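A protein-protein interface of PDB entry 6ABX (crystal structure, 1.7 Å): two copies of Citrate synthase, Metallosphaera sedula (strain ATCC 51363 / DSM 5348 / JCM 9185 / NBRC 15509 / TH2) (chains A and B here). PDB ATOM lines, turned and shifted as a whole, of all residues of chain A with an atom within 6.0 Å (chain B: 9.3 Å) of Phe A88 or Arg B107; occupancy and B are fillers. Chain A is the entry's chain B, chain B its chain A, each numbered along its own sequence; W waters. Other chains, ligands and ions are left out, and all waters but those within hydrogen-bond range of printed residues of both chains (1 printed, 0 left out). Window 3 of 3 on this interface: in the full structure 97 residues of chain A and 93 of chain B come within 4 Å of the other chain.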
ATOM      1  N   ARG A  84      23.064  23.012 -22.547  1.00  0.00           N
ATOM      2  CA  ARG A  84      21.888  23.776 -22.152  1.00  0.00           C
ATOM      3  C   ARG A  84      22.255  24.885 -21.171  1.00  0.00           C
ATOM      4  O   ARG A  84      21.587  25.890 -21.147  1.00  0.00           O
ATOM      5  CB  ARG A  84      20.816  22.814 -21.607  1.00  0.00           C
ATOM      6  CG  ARG A  84      19.633  23.468 -20.906  1.00  0.00           C
ATOM      7  CD  ARG A  84      18.668  22.434 -20.343  1.00  0.00           C
ATOM      8  NE  ARG A  84      17.284  22.875 -20.449  1.00  0.00           N
ATOM      9  CZ  ARG A  84      16.453  22.530 -21.434  1.00  0.00           C
ATOM     10  NH1 ARG A  84      15.192  22.919 -21.405  1.00  0.00           N
ATOM     11  NH2 ARG A  84      16.887  21.787 -22.440  1.00  0.00           N
ATOM     12  N   THR A  85      23.311  24.711 -20.342  1.00  0.00           N
ATOM     13  CA  THR A  85      23.605  25.600 -19.215  1.00  0.00           C
ATOM     14  C   THR A  85      24.859  26.461 -19.426  1.00  0.00           C
ATOM     15  O   THR A  85      25.051  27.392 -18.698  1.00  0.00           O
ATOM     16  CB  THR A  85      23.727  24.812 -17.899  1.00  0.00           C
ATOM     17  OG1 THR A  85      24.734  23.796 -18.004  1.00  0.00           O
ATOM     18  CG2 THR A  85      22.418  24.140 -17.557  1.00  0.00           C
ATOM     19  N   ALA A  86      25.701  26.167 -20.423  1.00  0.00           N
ATOM     20  CA  ALA A  86      27.000  26.723 -20.519  1.00  0.00           C
ATOM     21  C   ALA A  86      27.002  28.241 -20.769  1.00  0.00           C
ATOM     22  O   ALA A  86      27.898  28.972 -20.319  1.00  0.00           O
ATOM     23  CB  ALA A  86      27.781  25.996 -21.577  1.00  0.00           C
ATOM     24  N   LYS A  87      26.037  28.756 -21.509  1.00  0.00           N
ATOM     25  CA  LYS A  87      26.077  30.203 -21.847  1.00  0.00           C
ATOM     26  C   LYS A  87      25.812  31.096 -20.632  1.00  0.00           C
ATOM     27  O   LYS A  87      26.440  32.123 -20.488  1.00  0.00           O
ATOM     28  CB  LYS A  87      25.087  30.488 -22.973  1.00  0.00           C
ATOM     29  CG  LYS A  87      25.592  30.050 -24.337  1.00  0.00           C
ATOM     30  CD  LYS A  87      24.840  30.664 -25.486  1.00  0.00           C
ATOM     31  CE  LYS A  87      25.514  30.415 -26.817  1.00  0.00           C
ATOM     32  NZ  LYS A  87      25.120  31.467 -27.788  1.00  0.00           N
ATOM     33  N   PHE A  88      24.890  30.700 -19.751  1.00  0.00           N
ATOM     34  CA  PHE A  88      24.483  31.542 -18.630  1.00  0.00           C
ATOM     35  C   PHE A  88      25.050  31.035 -17.281  1.00  0.00           C
ATOM     36  O   PHE A  88      25.191  31.809 -16.375  1.00  0.00           O
ATOM     37  CB  PHE A  88      22.960  31.698 -18.671  1.00  0.00           C
ATOM     38  CG  PHE A  88      22.485  32.403 -19.922  1.00  0.00           C
ATOM     39  CD1 PHE A  88      22.820  33.735 -20.155  1.00  0.00           C
ATOM     40  CD2 PHE A  88      21.771  31.723 -20.899  1.00  0.00           C
ATOM     41  CE1 PHE A  88      22.425  34.374 -21.322  1.00  0.00           C
ATOM     42  CE2 PHE A  88      21.380  32.362 -22.067  1.00  0.00           C
ATOM     43  CZ  PHE A  88      21.709  33.686 -22.275  1.00  0.00           C
ATOM     44  N   GLY A  89      25.463  29.769 -17.178  1.00  0.00           N
ATOM     45  CA  GLY A  89      25.732  29.194 -15.862  1.00  0.00           C
ATOM     46  C   GLY A  89      27.166  29.409 -15.403  1.00  0.00           C
ATOM     47  O   GLY A  89      28.102  29.490 -16.200  1.00  0.00           O
ATOM     48  N   ASN A  90      27.340  29.493 -14.086  1.00  0.00           N
ATOM     49  CA  ASN A  90      28.700  29.535 -13.491  1.00  0.00           C
ATOM     50  C   ASN A  90      29.422  28.219 -13.813  1.00  0.00           C
ATOM     51  O   ASN A  90      28.850  27.141 -13.591  1.00  0.00           O
ATOM     52  CB  ASN A  90      28.600  29.739 -11.995  1.00  0.00           C
ATOM     53  CG  ASN A  90      29.947  29.625 -11.317  1.00  0.00           C
ATOM     54  OD1 ASN A  90      30.356  28.529 -10.943  1.00  0.00           O
ATOM     55  ND2 ASN A  90      30.608  30.750 -11.097  1.00  0.00           N
ATOM     56  N   ASP B  77      13.517  21.766 -15.576  1.00  0.00           N
ATOM     57  CA  ASP B  77      14.751  21.016 -15.690  1.00  0.00           C
ATOM     58  C   ASP B  77      14.864  20.053 -14.500  1.00  0.00           C
ATOM     59  O   ASP B  77      15.245  18.866 -14.627  1.00  0.00           O
ATOM     60  CB  ASP B  77      15.963  21.932 -15.760  1.00  0.00           C
ATOM     61  CG  ASP B  77      16.251  22.403 -17.176  1.00  0.00           C
ATOM     62  OD1 ASP B  77      15.369  22.194 -18.063  1.00  0.00           O
ATOM     63  OD2 ASP B  77      17.345  22.971 -17.377  1.00  0.00           O
ATOM     64  N   MET B 101      21.680  21.843  -9.112  1.00  0.00           N
ATOM     65  CA  MET B 101      20.990  22.488 -10.238  1.00  0.00           C
ATOM     66  C   MET B 101      20.278  23.760  -9.794  1.00  0.00           C
ATOM     67  O   MET B 101      20.329  24.764 -10.484  1.00  0.00           O
ATOM     68  CB  MET B 101      19.989  21.556 -10.914  1.00  0.00           C
ATOM     69  CG  MET B 101      20.616  20.411 -11.572  1.00  0.00           C
ATOM     70  SD  MET B 101      19.409  19.115 -12.072  1.00  0.00           S
ATOM     71  CE  MET B 101      18.488  19.955 -13.358  1.00  0.00           C
ATOM     72  N   MET B 102      19.646  23.736  -8.630  1.00  0.00           N
ATOM     73  CA  MET B 102      18.986  24.890  -8.092  1.00  0.00           C
ATOM     74  C   MET B 102      19.955  26.078  -7.967  1.00  0.00           C
ATOM     75  O   MET B 102      19.613  27.228  -8.316  1.00  0.00           O
ATOM     76  CB  MET B 102      18.425  24.504  -6.710  1.00  0.00           C
ATOM     77  CG  MET B 102      17.112  25.025  -6.370  1.00  0.00           C
ATOM     78  SD  MET B 102      16.851  24.444  -4.636  1.00  0.00           S
ATOM     79  CE  MET B 102      16.089  22.858  -4.932  1.00  0.00           C
ATOM     80  N   GLY B 103      21.162  25.815  -7.440  1.00  0.00           N
ATOM     81  CA  GLY B 103      22.226  26.783  -7.264  1.00  0.00           C
ATOM     82  C   GLY B 103      22.688  27.345  -8.623  1.00  0.00           C
ATOM     83  O   GLY B 103      22.883  28.532  -8.777  1.00  0.00           O
ATOM     84  N   LEU B 104      22.884  26.456  -9.600  1.00  0.00           N
ATOM     85  CA  LEU B 104      23.306  26.799 -10.933  1.00  0.00           C
ATOM     86  C   LEU B 104      22.276  27.727 -11.566  1.00  0.00           C
ATOM     87  O   LEU B 104      22.643  28.713 -12.184  1.00  0.00           O
ATOM     88  CB  LEU B 104      23.454  25.508 -11.738  1.00  0.00           C
ATOM     89  CG  LEU B 104      23.706  25.648 -13.244  1.00  0.00           C
ATOM     90  CD1 LEU B 104      24.931  26.447 -13.549  1.00  0.00           C
ATOM     91  CD2 LEU B 104      23.850  24.266 -13.869  1.00  0.00           C
ATOM     92  N   GLU B 105      20.993  27.453 -11.299  1.00  0.00           N
ATOM     93  CA  GLU B 105      19.890  28.177 -11.915  1.00  0.00           C
ATOM     94  C   GLU B 105      19.651  29.535 -11.224  1.00  0.00           C
ATOM     95  O   GLU B 105      18.983  30.366 -11.817  1.00  0.00           O
ATOM     96  CB  GLU B 105      18.624  27.293 -11.954  1.00  0.00           C
ATOM     97  CG  GLU B 105      18.710  26.123 -12.921  1.00  0.00           C
ATOM     98  CD  GLU B 105      17.720  24.949 -12.797  1.00  0.00           C
ATOM     99  OE1 GLU B 105      16.702  25.114 -12.121  1.00  0.00           O
ATOM    100  OE2 GLU B 105      17.982  23.832 -13.388  1.00  0.00           O
ATOM    101  N   ASP B 106      20.147  29.768  -9.995  1.00  0.00           N
ATOM    102  CA  ASP B 106      19.882  30.979  -9.279  1.00  0.00           C
ATOM    103  C   ASP B 106      21.045  31.958  -9.459  1.00  0.00           C
ATOM    104  O   ASP B 106      22.022  31.921  -8.739  1.00  0.00           O
ATOM    105  CB  ASP B 106      19.554  30.698  -7.809  1.00  0.00           C
ATOM    106  CG  ASP B 106      19.193  31.924  -6.999  1.00  0.00           C
ATOM    107  OD1 ASP B 106      19.245  33.029  -7.586  1.00  0.00           O
ATOM    108  OD2 ASP B 106      18.896  31.770  -5.767  1.00  0.00           O
ATOM    109  N   ARG B 107      20.826  32.928 -10.352  1.00  0.00           N
ATOM    110  CA  ARG B 107      21.869  33.857 -10.765  1.00  0.00           C
ATOM    111  C   ARG B 107      21.852  35.114  -9.884  1.00  0.00           C
ATOM    112  O   ARG B 107      22.723  35.965 -10.058  1.00  0.00           O
ATOM    113  CB  ARG B 107      21.714  34.146 -12.262  1.00  0.00           C
ATOM    114  CG  ARG B 107      21.873  32.894 -13.121  1.00  0.00           C
ATOM    115  CD  ARG B 107      22.290  33.131 -14.564  1.00  0.00           C
ATOM    116  NE  ARG B 107      21.174  33.482 -15.445  1.00  0.00           N
ATOM    117  CZ  ARG B 107      20.243  32.633 -15.882  1.00  0.00           C
ATOM    118  NH1 ARG B 107      20.143  31.422 -15.360  1.00  0.00           N
ATOM    119  NH2 ARG B 107      19.417  32.997 -16.847  1.00  0.00           N
ATOM    120  N   SER B 108      20.922  35.210  -8.922  1.00  0.00           N
ATOM    121  CA  SER B 108      20.863  36.375  -8.002  1.00  0.00           C
ATOM    122  C   SER B 108      22.117  36.390  -7.110  1.00  0.00           C
ATOM    123  O   SER B 108      22.737  35.331  -6.893  1.00  0.00           O
ATOM    124  CB  SER B 108      19.612  36.357  -7.198  1.00  0.00           C
ATOM    125  OG  SER B 108      19.676  35.297  -6.256  1.00  0.00           O
ATOM    126  N   GLU B 109      22.477  37.578  -6.596  1.00  0.00           N
ATOM    127  CA  GLU B 109      23.686  37.760  -5.736  1.00  0.00           C
ATOM    128  C   GLU B 109      23.295  37.979  -4.266  1.00  0.00           C
ATOM    129  O   GLU B 109      22.261  38.595  -3.973  1.00  0.00           O
ATOM    130  CB  GLU B 109      24.526  38.951  -6.206  1.00  0.00           C
ATOM    131  CG  GLU B 109      25.962  38.921  -5.696  1.00  0.00           C
ATOM    132  CD  GLU B 109      26.659  37.573  -5.848  1.00  0.00           C
ATOM    133  OE1 GLU B 109      27.422  37.413  -6.826  1.00  0.00           O
ATOM    134  OE2 GLU B 109      26.441  36.676  -4.980  1.00  0.00           O
ATOM    135  N   GLY B 110      24.162  37.513  -3.346  1.00  0.00           N
ATOM    136  CA  GLY B 110      23.942  37.632  -1.914  1.00  0.00           C
ATOM    137  C   GLY B 110      22.676  36.892  -1.460  1.00  0.00           C
ATOM    138  O   GLY B 110      22.372  35.766  -1.950  1.00  0.00           O
ATOM    139  N   LYS B 115      17.965  32.492  -0.142  1.00  0.00           N
ATOM    140  CA  LYS B 115      18.323  31.230  -0.830  1.00  0.00           C
ATOM    141  C   LYS B 115      18.061  30.035   0.077  1.00  0.00           C
ATOM    142  O   LYS B 115      17.586  29.003  -0.406  1.00  0.00           O
ATOM    143  CB  LYS B 115      19.760  31.307  -1.352  1.00  0.00           C
ATOM    144  CG  LYS B 115      19.916  32.282  -2.507  1.00  0.00           C
ATOM    145  CD  LYS B 115      21.353  32.649  -2.815  1.00  0.00           C
ATOM    146  CE  LYS B 115      21.438  33.528  -4.042  1.00  0.00           C
ATOM    147  NZ  LYS B 115      22.796  34.062  -4.225  1.00  0.00           N
ATOM    148  N   LYS B 118      14.402  29.366  -0.186  1.00  0.00           N
ATOM    149  CA  LYS B 118      14.093  28.663  -1.401  1.00  0.00           C
ATOM    150  C   LYS B 118      14.381  27.161  -1.271  1.00  0.00           C
ATOM    151  O   LYS B 118      13.572  26.305  -1.664  1.00  0.00           O
ATOM    152  CB  LYS B 118      14.833  29.272  -2.586  1.00  0.00           C
ATOM    153  CG  LYS B 118      14.227  30.592  -3.052  1.00  0.00           C
ATOM    154  CD  LYS B 118      14.996  31.214  -4.169  1.00  0.00           C
ATOM    155  CE  LYS B 118      14.184  32.343  -4.773  1.00  0.00           C
ATOM    156  NZ  LYS B 118      14.957  33.062  -5.805  1.00  0.00           N
ATOM    157  N   TYR B 199      24.386  27.607  -1.745  1.00  0.00           N
ATOM    158  CA  TYR B 199      23.990  26.328  -2.394  1.00  0.00           C
ATOM    159  C   TYR B 199      25.139  25.330  -2.388  1.00  0.00           C
ATOM    160  O   TYR B 199      24.905  24.147  -2.085  1.00  0.00           O
ATOM    161  CB  TYR B 199      23.447  26.521  -3.809  1.00  0.00           C
ATOM    162  CG  TYR B 199      22.150  27.273  -3.948  1.00  0.00           C
ATOM    163  CD1 TYR B 199      20.914  26.648  -3.835  1.00  0.00           C
ATOM    164  CD2 TYR B 199      22.152  28.636  -4.221  1.00  0.00           C
ATOM    165  CE1 TYR B 199      19.725  27.332  -4.054  1.00  0.00           C
ATOM    166  CE2 TYR B 199      20.978  29.330  -4.444  1.00  0.00           C
ATOM    167  CZ  TYR B 199      19.756  28.685  -4.363  1.00  0.00           C
ATOM    168  OH  TYR B 199      18.612  29.400  -4.601  1.00  0.00           O
HETATM  169  O   HOH W   1      25.192  29.706 -12.149  1.00  0.00           O
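Phe A88 touches one residue of chain B.
Of the printed residues of chain A, Arg B107 touches Phe A88.
Of chain B, only Leu B104 comes within 4 Å of Gly A89.
Printed residues of chain B within 4 Å of Thr A85: Leu B104 (3.96 Å).
Of the printed residues of chain B, Asn A90 touches Leu B104 (3.9 Å).
Of the printed residues of chain B, Arg A84 touches Asp B77 (3.1 Å).
Lys A87 touches none of the printed residues of chain B.
Met B102 touches none of the printed residues of chain A.
The nearest printed residue of chain B that does not touch Asn A90 is Arg B107 (6.2 Å).
Of the 14 printed residues of chain B, 3 touch a printed residue of chain A.
Hydrophobic or aromatic side chains of chain B within 4 Å of the printed part of chain A: Leu B104.
Printed residues of chain A that touch a printed residue of chain B: Arg A84, Thr A85, Phe A88, Gly A89 and Asn A90.
Among the printed residues, 5 pairs touch across the chains.
No position is printed for both chains.
Of the 5 pairs that touch across the chains among the printed residues, none has its exchanged pair printed and touching as well.
Among the printed residues, pairs that only touch across the chains: Phe A88 with Arg B107, Gly A89 with Leu B104, Asn A90 with Leu B104 and Thr A85 with Leu B104.
Water W1 lies within hydrogen-bond range of O of Leu B104 and N of Asn A90.
The side-chain carboxylate (OD2) of Asp B77 is in salt-bridge range of the guanidinium group (NE) of Arg A84 (3.1 Å).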
